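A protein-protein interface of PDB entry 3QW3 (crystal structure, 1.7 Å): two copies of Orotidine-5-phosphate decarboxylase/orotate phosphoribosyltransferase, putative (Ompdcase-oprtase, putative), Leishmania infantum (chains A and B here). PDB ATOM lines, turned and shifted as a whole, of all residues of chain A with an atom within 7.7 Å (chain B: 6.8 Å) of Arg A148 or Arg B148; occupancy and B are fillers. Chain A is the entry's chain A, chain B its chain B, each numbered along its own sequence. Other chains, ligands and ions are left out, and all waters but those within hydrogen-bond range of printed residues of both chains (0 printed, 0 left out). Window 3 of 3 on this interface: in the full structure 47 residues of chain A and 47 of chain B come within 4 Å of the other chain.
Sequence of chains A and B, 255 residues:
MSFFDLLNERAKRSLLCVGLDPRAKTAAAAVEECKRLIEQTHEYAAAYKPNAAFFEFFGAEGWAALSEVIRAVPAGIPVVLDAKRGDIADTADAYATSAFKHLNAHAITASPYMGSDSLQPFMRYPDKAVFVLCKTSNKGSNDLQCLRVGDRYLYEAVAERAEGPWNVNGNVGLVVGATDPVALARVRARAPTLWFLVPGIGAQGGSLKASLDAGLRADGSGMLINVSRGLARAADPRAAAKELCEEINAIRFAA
Asn A142 touches none of the printed residues of chain B. Printed residues of chain B within 4 Å of Leu A147: Val B149 and Leu B154. Printed residues of chain B within 4 Å of Arg A148: Arg B148 and Val B149. Gly A150 touches none of the printed residues of chain B. Printed residues of chain A within 4 Å of Leu B147: Val A149 (3.8 Å) and Leu A154 (3.7 Å). Of the printed residues of chain A, Arg B148 touches Arg A148 and Val A149. Printed residues of chain A within 4 Å of Leu B154: Leu A147 (3.9 Å) and Leu A154 (3.98 Å). The nearest printed residue of chain A that does not touch Arg B148 is Gly A150 (4.3 Å). The nearest printed residue of chain B that does not touch Leu A154 is Leu B144 (4.3 Å).
Leu A147 touches Leu B154, and with the chains exchanged Leu A154 touches Leu B147. Arg A148 touches its own counterpart, Arg B148. Arg A148 touches Val B149, and with the chains exchanged Val A149 touches Arg B148. Val A149 touches its own counterpart, Val B149. Positions printed for both chains: 144, 145, 146, 147, 148, 149, 150, 151, 152, 153 and 154. Of the 9 pairs that touch across the chains among the printed residues, 9 have their exchanged pair printed and touching as well.
Among the printed residues, merely in contact across the chains: Arg A148 with Val B149, Val A149 with Arg B148, Arg A148 with Arg B148, Leu A154 with Leu B147, Val A149 with Val B149, Val A149 with Leu B147, Leu A147 with Val B149, Leu A147 with Leu B154 and Leu A154 with Leu B154.
The backbone NH of Leu A154 is in hydrogen-bond range of the backbone carbonyl oxygen of Gln A145 (3.3 Å). The guanidinium group (NH1) of Arg B152 sits at hydrogen-bond distance from the backbone carbonyl oxygen (O) of Val B149 (3.0 Å). The backbone carbonyl oxygen (O) of Asp B151 lies within hydrogen-bond range of the guanidinium group (NH1) of Arg B148. The backbone carbonyl oxygen of Leu B147 lies within hydrogen-bond range of the backbone NH of Leu B154, 2.8 Å away. N of Leu A154 lies within hydrogen-bond range of O of Leu A147. O of Gln B145 is in hydrogen-bond range of N of Leu B154 (3.3 Å).
Of the 13 printed residues of chain B, 4 touch a printed residue of chain A. Printed residues of chain B that touch a printed residue of chain A: Leu B147, Arg B148, Val B149 and Leu B154. Hydrophobic or aromatic side chains of chain B within 4 Å of the printed part of chain A: Leu B147, Val B149 and Leu B154. Of the 13 printed residues of chain A, 4 touch a printed residue of chain B. Hydrophobic or aromatic side chains of chain A within 4 Å of the printed part of chain B: Leu A147, Val A149 and Leu A154. Along chain A the printed residues that touch a printed residue of chain B span positions 147 to 154. Among the printed residues, no Asp or Glu carboxylate lies within 4 Å of a Lys or Arg side-chain nitrogen of the other chain.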
ATOM      1  N   ASN A 142     -18.046  -0.004  -2.486  1.00  0.00           N
ATOM      2  CA  ASN A 142     -19.012  -0.658  -1.606  1.00  0.00           C
ATOM      3  C   ASN A 142     -18.411  -1.827  -0.827  1.00  0.00           C
ATOM      4  O   ASN A 142     -18.819  -2.100   0.306  1.00  0.00           O
ATOM      5  N   LEU A 144     -15.376  -2.554   0.606  1.00  0.00           N
ATOM      6  CA  LEU A 144     -14.589  -2.368   1.822  1.00  0.00           C
ATOM      7  C   LEU A 144     -14.800  -0.992   2.436  1.00  0.00           C
ATOM      8  O   LEU A 144     -15.049  -0.879   3.633  1.00  0.00           O
ATOM      9  CB  LEU A 144     -13.094  -2.589   1.555  1.00  0.00           C
ATOM     10  CG  LEU A 144     -12.502  -4.003   1.591  1.00  0.00           C
ATOM     11  CD1 LEU A 144     -12.882  -4.816   0.357  1.00  0.00           C
ATOM     12  CD2 LEU A 144     -10.990  -3.927   1.724  1.00  0.00           C
ATOM     13  N   GLN A 145     -14.696   0.049   1.610  1.00  0.00           N
ATOM     14  CA  GLN A 145     -14.717   1.430   2.101  1.00  0.00           C
ATOM     15  C   GLN A 145     -15.999   1.783   2.857  1.00  0.00           C
ATOM     16  O   GLN A 145     -15.962   2.525   3.839  1.00  0.00           O
ATOM     17  CB  GLN A 145     -14.513   2.409   0.942  1.00  0.00           C
ATOM     18  CG  GLN A 145     -13.122   2.363   0.333  1.00  0.00           C
ATOM     19  CD  GLN A 145     -13.042   3.098  -0.986  1.00  0.00           C
ATOM     20  OE1 GLN A 145     -13.825   4.015  -1.247  1.00  0.00           O
ATOM     21  NE2 GLN A 145     -12.089   2.709  -1.825  1.00  0.00           N
ATOM     22  N   CYS A 146     -17.124   1.243   2.393  1.00  0.00           N
ATOM     23  CA  CYS A 146     -18.424   1.571   2.970  1.00  0.00           C
ATOM     24  C   CYS A 146     -18.917   0.539   3.984  1.00  0.00           C
ATOM     25  O   CYS A 146     -20.078   0.580   4.403  1.00  0.00           O
ATOM     26  CB  CYS A 146     -19.459   1.804   1.866  1.00  0.00           C
ATOM     27  SG  CYS A 146     -19.088   3.232   0.829  1.00  0.00           S
ATOM     28  N   LEU A 147     -18.036  -0.381   4.377  1.00  0.00           N
ATOM     29  CA  LEU A 147     -18.322  -1.286   5.489  1.00  0.00           C
ATOM     30  C   LEU A 147     -18.369  -0.489   6.787  1.00  0.00           C
ATOM     31  O   LEU A 147     -17.660   0.511   6.940  1.00  0.00           O
ATOM     32  CB  LEU A 147     -17.283  -2.406   5.587  1.00  0.00           C
ATOM     33  CG  LEU A 147     -17.268  -3.463   4.476  1.00  0.00           C
ATOM     34  CD1 LEU A 147     -16.105  -4.428   4.677  1.00  0.00           C
ATOM     35  CD2 LEU A 147     -18.589  -4.219   4.411  1.00  0.00           C
ATOM     36  N   ARG A 148     -19.209  -0.941   7.713  1.00  0.00           N
ATOM     37  CA  ARG A 148     -19.419  -0.254   8.980  1.00  0.00           C
ATOM     38  C   ARG A 148     -18.468  -0.744  10.068  1.00  0.00           C
ATOM     39  O   ARG A 148     -18.446  -1.932  10.399  1.00  0.00           O
ATOM     40  CB  ARG A 148     -20.874  -0.421   9.429  1.00  0.00           C
ATOM     41  CG  ARG A 148     -21.161   0.117  10.818  1.00  0.00           C
ATOM     42  CD  ARG A 148     -22.656   0.209  11.085  1.00  0.00           C
ATOM     43  NE  ARG A 148     -22.937   0.879  12.350  1.00  0.00           N
ATOM     44  CZ  ARG A 148     -24.133   1.336  12.706  1.00  0.00           C
ATOM     45  NH1 ARG A 148     -25.169   1.201  11.890  1.00  0.00           N
ATOM     46  NH2 ARG A 148     -24.291   1.935  13.878  1.00  0.00           N
ATOM     47  N   VAL A 149     -17.677   0.180  10.610  1.00  0.00           N
ATOM     48  CA  VAL A 149     -16.822  -0.101  11.766  1.00  0.00           C
ATOM     49  C   VAL A 149     -17.362   0.732  12.926  1.00  0.00           C
ATOM     50  O   VAL A 149     -17.197   1.956  12.957  1.00  0.00           O
ATOM     51  CB  VAL A 149     -15.335   0.251  11.497  1.00  0.00           C
ATOM     52  CG1 VAL A 149     -14.494   0.046  12.751  1.00  0.00           C
ATOM     53  CG2 VAL A 149     -14.786  -0.582  10.346  1.00  0.00           C
ATOM     54  N   GLY A 150     -18.029   0.068  13.866  1.00  0.00           N
ATOM     55  CA  GLY A 150     -18.707   0.766  14.960  1.00  0.00           C
ATOM     56  C   GLY A 150     -19.802   1.668  14.424  1.00  0.00           C
ATOM     57  O   GLY A 150     -20.722   1.203  13.753  1.00  0.00           O
ATOM     58  N   ASP A 151     -19.689   2.964  14.704  1.00  0.00           N
ATOM     59  CA  ASP A 151     -20.681   3.937  14.254  1.00  0.00           C
ATOM     60  C   ASP A 151     -20.196   4.765  13.064  1.00  0.00           C
ATOM     61  O   ASP A 151     -20.657   5.888  12.857  1.00  0.00           O
ATOM     62  N   ARG A 152     -19.273   4.210  12.282  1.00  0.00           N
ATOM     63  CA  ARG A 152     -18.748   4.912  11.105  1.00  0.00           C
ATOM     64  C   ARG A 152     -18.304   3.963   9.995  1.00  0.00           C
ATOM     65  O   ARG A 152     -18.173   2.762  10.211  1.00  0.00           O
ATOM     66  CB  ARG A 152     -17.614   5.867  11.504  1.00  0.00           C
ATOM     67  CG  ARG A 152     -16.345   5.196  11.984  1.00  0.00           C
ATOM     68  CD  ARG A 152     -15.698   6.011  13.089  1.00  0.00           C
ATOM     69  NE  ARG A 152     -14.274   5.713  13.227  1.00  0.00           N
ATOM     70  CZ  ARG A 152     -13.770   4.685  13.906  1.00  0.00           C
ATOM     71  NH1 ARG A 152     -14.566   3.826  14.526  1.00  0.00           N
ATOM     72  NH2 ARG A 152     -12.457   4.517  13.960  1.00  0.00           N
ATOM     73  N   TYR A 153     -18.086   4.516   8.806  1.00  0.00           N
ATOM     74  CA  TYR A 153     -17.618   3.742   7.665  1.00  0.00           C
ATOM     75  C   TYR A 153     -16.113   3.515   7.754  1.00  0.00           C
ATOM     76  O   TYR A 153     -15.401   4.291   8.398  1.00  0.00           O
ATOM     77  CB  TYR A 153     -17.953   4.469   6.363  1.00  0.00           C
ATOM     78  CG  TYR A 153     -19.432   4.648   6.118  1.00  0.00           C
ATOM     79  CD1 TYR A 153     -20.229   3.566   5.747  1.00  0.00           C
ATOM     80  CD2 TYR A 153     -20.036   5.897   6.255  1.00  0.00           C
ATOM     81  CE1 TYR A 153     -21.590   3.720   5.519  1.00  0.00           C
ATOM     82  CE2 TYR A 153     -21.402   6.065   6.031  1.00  0.00           C
ATOM     83  CZ  TYR A 153     -22.169   4.972   5.661  1.00  0.00           C
ATOM     84  OH  TYR A 153     -23.519   5.120   5.433  1.00  0.00           O
ATOM     85  N   LEU A 154     -15.629   2.456   7.106  1.00  0.00           N
ATOM     86  CA  LEU A 154     -14.187   2.191   7.061  1.00  0.00           C
ATOM     87  C   LEU A 154     -13.409   3.412   6.566  1.00  0.00           C
ATOM     88  O   LEU A 154     -12.332   3.719   7.084  1.00  0.00           O
ATOM     89  CB  LEU A 154     -13.853   0.961   6.199  1.00  0.00           C
ATOM     90  CG  LEU A 154     -12.354   0.650   6.020  1.00  0.00           C
ATOM     91  CD1 LEU A 154     -11.712   0.218   7.338  1.00  0.00           C
ATOM     92  CD2 LEU A 154     -12.088  -0.393   4.936  1.00  0.00           C
ATOM     93  N   TYR A 155     -13.953   4.117   5.576  1.00  0.00           N
ATOM     94  CA  TYR A 155     -13.242   5.281   5.038  1.00  0.00           C
ATOM     95  C   TYR A 155     -13.089   6.409   6.057  1.00  0.00           C
ATOM     96  O   TYR A 155     -12.092   7.129   6.046  1.00  0.00           O
ATOM     97  CB  TYR A 155     -13.835   5.769   3.707  1.00  0.00           C
ATOM     98  CG  TYR A 155     -15.208   6.411   3.762  1.00  0.00           C
ATOM     99  CD1 TYR A 155     -16.341   5.698   3.390  1.00  0.00           C
ATOM    100  CD2 TYR A 155     -15.362   7.749   4.132  1.00  0.00           C
ATOM    101  CE1 TYR A 155     -17.600   6.285   3.407  1.00  0.00           C
ATOM    102  CE2 TYR A 155     -16.617   8.348   4.157  1.00  0.00           C
ATOM    103  CZ  TYR A 155     -17.732   7.606   3.793  1.00  0.00           C
ATOM    104  OH  TYR A 155     -18.981   8.178   3.806  1.00  0.00           O
ATOM    105  N   LEU B 144      -6.182  -1.453   9.914  1.00  0.00           N
ATOM    106  CA  LEU B 144      -7.368  -1.672   9.112  1.00  0.00           C
ATOM    107  C   LEU B 144      -7.818  -3.125   9.191  1.00  0.00           C
ATOM    108  O   LEU B 144      -8.989  -3.396   9.434  1.00  0.00           O
ATOM    109  CB  LEU B 144      -7.132  -1.261   7.652  1.00  0.00           C
ATOM    110  CG  LEU B 144      -7.391   0.196   7.231  1.00  0.00           C
ATOM    111  CD1 LEU B 144      -6.305   1.132   7.716  1.00  0.00           C
ATOM    112  CD2 LEU B 144      -7.551   0.315   5.719  1.00  0.00           C
ATOM    113  N   GLN B 145      -6.878  -4.048   9.001  1.00  0.00           N
ATOM    114  CA  GLN B 145      -7.214  -5.468   8.819  1.00  0.00           C
ATOM    115  C   GLN B 145      -7.966  -6.089   9.996  1.00  0.00           C
ATOM    116  O   GLN B 145      -8.815  -6.963   9.801  1.00  0.00           O
ATOM    117  CB  GLN B 145      -5.955  -6.282   8.506  1.00  0.00           C
ATOM    118  CG  GLN B 145      -5.358  -5.960   7.141  1.00  0.00           C
ATOM    119  CD  GLN B 145      -3.955  -6.503   6.957  1.00  0.00           C
ATOM    120  OE1 GLN B 145      -3.553  -7.467   7.606  1.00  0.00           O
ATOM    121  NE2 GLN B 145      -3.201  -5.879   6.070  1.00  0.00           N
ATOM    122  N   CYS B 146      -7.655  -5.633  11.208  1.00  0.00           N
ATOM    123  CA  CYS B 146      -8.267  -6.187  12.417  1.00  0.00           C
ATOM    124  C   CYS B 146      -9.423  -5.357  12.986  1.00  0.00           C
ATOM    125  O   CYS B 146      -9.927  -5.647  14.079  1.00  0.00           O
ATOM    126  CB  CYS B 146      -7.204  -6.453  13.482  1.00  0.00           C
ATOM    127  SG  CYS B 146      -6.070  -7.774  13.017  1.00  0.00           S
ATOM    128  N   LEU B 147      -9.843  -4.339  12.240  1.00  0.00           N
ATOM    129  CA  LEU B 147     -11.084  -3.626  12.540  1.00  0.00           C
ATOM    130  C   LEU B 147     -12.272  -4.571  12.425  1.00  0.00           C
ATOM    131  O   LEU B 147     -12.299  -5.441  11.553  1.00  0.00           O
ATOM    132  CB  LEU B 147     -11.276  -2.443  11.592  1.00  0.00           C
ATOM    133  CG  LEU B 147     -10.940  -1.023  12.067  1.00  0.00           C
ATOM    134  CD1 LEU B 147      -9.880  -0.967  13.169  1.00  0.00           C
ATOM    135  CD2 LEU B 147     -10.560  -0.151  10.880  1.00  0.00           C
ATOM    136  N   ARG B 148     -13.244  -4.398  13.317  1.00  0.00           N
ATOM    137  CA  ARG B 148     -14.441  -5.236  13.320  1.00  0.00           C
ATOM    138  C   ARG B 148     -15.506  -4.649  12.409  1.00  0.00           C
ATOM    139  O   ARG B 148     -15.932  -3.506  12.587  1.00  0.00           O
ATOM    140  CB  ARG B 148     -14.999  -5.400  14.741  1.00  0.00           C
ATOM    141  CG  ARG B 148     -14.032  -6.013  15.753  1.00  0.00           C
ATOM    142  CD  ARG B 148     -13.772  -7.493  15.490  1.00  0.00           C
ATOM    143  NE  ARG B 148     -14.964  -8.322  15.675  1.00  0.00           N
ATOM    144  CZ  ARG B 148     -15.015  -9.630  15.429  1.00  0.00           C
ATOM    145  NH1 ARG B 148     -16.142 -10.302  15.629  1.00  0.00           N
ATOM    146  NH2 ARG B 148     -13.939 -10.272  14.983  1.00  0.00           N
ATOM    147  N   VAL B 149     -15.919  -5.441  11.424  1.00  0.00           N
ATOM    148  CA  VAL B 149     -17.012  -5.078  10.533  1.00  0.00           C
ATOM    149  C   VAL B 149     -18.182  -6.024  10.800  1.00  0.00           C
ATOM    150  O   VAL B 149     -18.340  -7.056  10.142  1.00  0.00           O
ATOM    151  CB  VAL B 149     -16.574  -5.058   9.035  1.00  0.00           C
ATOM    152  CG1 VAL B 149     -15.690  -3.855   8.761  1.00  0.00           C
ATOM    153  CG2 VAL B 149     -15.837  -6.340   8.646  1.00  0.00           C
ATOM    154  N   GLY B 150     -18.985  -5.675  11.799  1.00  0.00           N
ATOM    155  CA  GLY B 150     -20.045  -6.556  12.277  1.00  0.00           C
ATOM    156  C   GLY B 150     -19.455  -7.642  13.155  1.00  0.00           C
ATOM    157  O   GLY B 150     -18.749  -7.349  14.127  1.00  0.00           O
ATOM    158  N   ASP B 151     -19.731  -8.893  12.797  1.00  0.00           N
ATOM    159  CA  ASP B 151     -19.264 -10.046  13.564  1.00  0.00           C
ATOM    160  C   ASP B 151     -17.993 -10.682  12.980  1.00  0.00           C
ATOM    161  O   ASP B 151     -17.688 -11.847  13.258  1.00  0.00           O
ATOM    162  CB  ASP B 151     -20.380 -11.093  13.683  1.00  0.00           C
ATOM    163  N   ARG B 152     -17.254  -9.923  12.175  1.00  0.00           N
ATOM    164  CA  ARG B 152     -15.976 -10.409  11.649  1.00  0.00           C
ATOM    165  C   ARG B 152     -14.940  -9.297  11.511  1.00  0.00           C
ATOM    166  O   ARG B 152     -15.273  -8.111  11.577  1.00  0.00           O
ATOM    167  CB  ARG B 152     -16.164 -11.161  10.321  1.00  0.00           C
ATOM    168  CG  ARG B 152     -16.431 -10.296   9.097  1.00  0.00           C
ATOM    169  CD  ARG B 152     -17.896 -10.316   8.700  1.00  0.00           C
ATOM    170  NE  ARG B 152     -18.055 -10.165   7.256  1.00  0.00           N
ATOM    171  CZ  ARG B 152     -18.548  -9.091   6.645  1.00  0.00           C
ATOM    172  NH1 ARG B 152     -18.964  -8.040   7.341  1.00  0.00           N
ATOM    173  NH2 ARG B 152     -18.640  -9.074   5.325  1.00  0.00           N
ATOM    174  N   TYR B 153     -13.682  -9.696  11.340  1.00  0.00           N
ATOM    175  CA  TYR B 153     -12.599  -8.756  11.073  1.00  0.00           C
ATOM    176  C   TYR B 153     -12.636  -8.340   9.611  1.00  0.00           C
ATOM    177  O   TYR B 153     -13.142  -9.085   8.763  1.00  0.00           O
ATOM    178  CB  TYR B 153     -11.246  -9.401  11.362  1.00  0.00           C
ATOM    179  CG  TYR B 153     -11.006  -9.752  12.810  1.00  0.00           C
ATOM    180  CD1 TYR B 153     -10.760  -8.756  13.755  1.00  0.00           C
ATOM    181  CD2 TYR B 153     -11.004 -11.078  13.232  1.00  0.00           C
ATOM    182  CE1 TYR B 153     -10.530  -9.073  15.089  1.00  0.00           C
ATOM    183  CE2 TYR B 153     -10.773 -11.409  14.565  1.00  0.00           C
ATOM    184  CZ  TYR B 153     -10.538 -10.402  15.485  1.00  0.00           C
ATOM    185  OH  TYR B 153     -10.313 -10.717  16.804  1.00  0.00           O
ATOM    186  N   LEU B 154     -12.084  -7.167   9.310  1.00  0.00           N
ATOM    187  CA  LEU B 154     -11.997  -6.707   7.921  1.00  0.00           C
ATOM    188  C   LEU B 154     -11.336  -7.748   7.013  1.00  0.00           C
ATOM    189  O   LEU B 154     -11.800  -7.979   5.892  1.00  0.00           O
ATOM    190  CB  LEU B 154     -11.256  -5.367   7.815  1.00  0.00           C
ATOM    191  CG  LEU B 154     -11.051  -4.819   6.391  1.00  0.00           C
ATOM    192  CD1 LEU B 154     -12.374  -4.543   5.695  1.00  0.00           C
ATOM    193  CD2 LEU B 154     -10.180  -3.565   6.402  1.00  0.00           C
ATOM    194  N   GLU B 156     -11.360 -10.912   7.257  1.00  0.00           N
ATOM    195  CA  GLU B 156     -12.345 -11.966   6.979  1.00  0.00           C
ATOM    196  C   GLU B 156     -13.348 -11.534   5.917  1.00  0.00           C
ATOM    197  O   GLU B 156     -13.759 -12.347   5.087  1.00  0.00           O
ATOM    198  CB  GLU B 156     -13.069 -12.406   8.253  1.00  0.00           C
ATOM    199  CG  GLU B 156     -12.192 -13.189   9.210  1.00  0.00           C
ATOM    200  CD  GLU B 156     -12.875 -13.452  10.540  1.00  0.00           C
ATOM    201  OE1 GLU B 156     -13.073 -14.636  10.877  1.00  0.00           O
ATOM    202  OE2 GLU B 156     -13.224 -12.478  11.244  1.00  0.00           O
ATOM    203  N   ARG B 186      -8.414 -18.602  10.620  1.00  0.00           N
ATOM    204  CA  ARG B 186      -9.676 -17.882  10.410  1.00  0.00           C
ATOM    205  C   ARG B 186      -9.940 -17.649   8.927  1.00  0.00           C
ATOM    206  O   ARG B 186     -11.073 -17.814   8.455  1.00  0.00           O
ATOM    207  CB  ARG B 186      -9.693 -16.536  11.148  1.00  0.00           C
ATOM    208  CG  ARG B 186      -9.857 -16.630  12.663  1.00  0.00           C
ATOM    209  CD  ARG B 186     -10.421 -15.319  13.216  1.00  0.00           C
ATOM    210  NE  ARG B 186     -10.380 -15.273  14.676  1.00  0.00           N
ATOM    211  CZ  ARG B 186      -9.394 -14.727  15.384  1.00  0.00           C
ATOM    212  NH1 ARG B 186      -8.354 -14.169  14.773  1.00  0.00           N
ATOM    213  NH2 ARG B 186      -9.446 -14.736  16.709  1.00  0.00           N
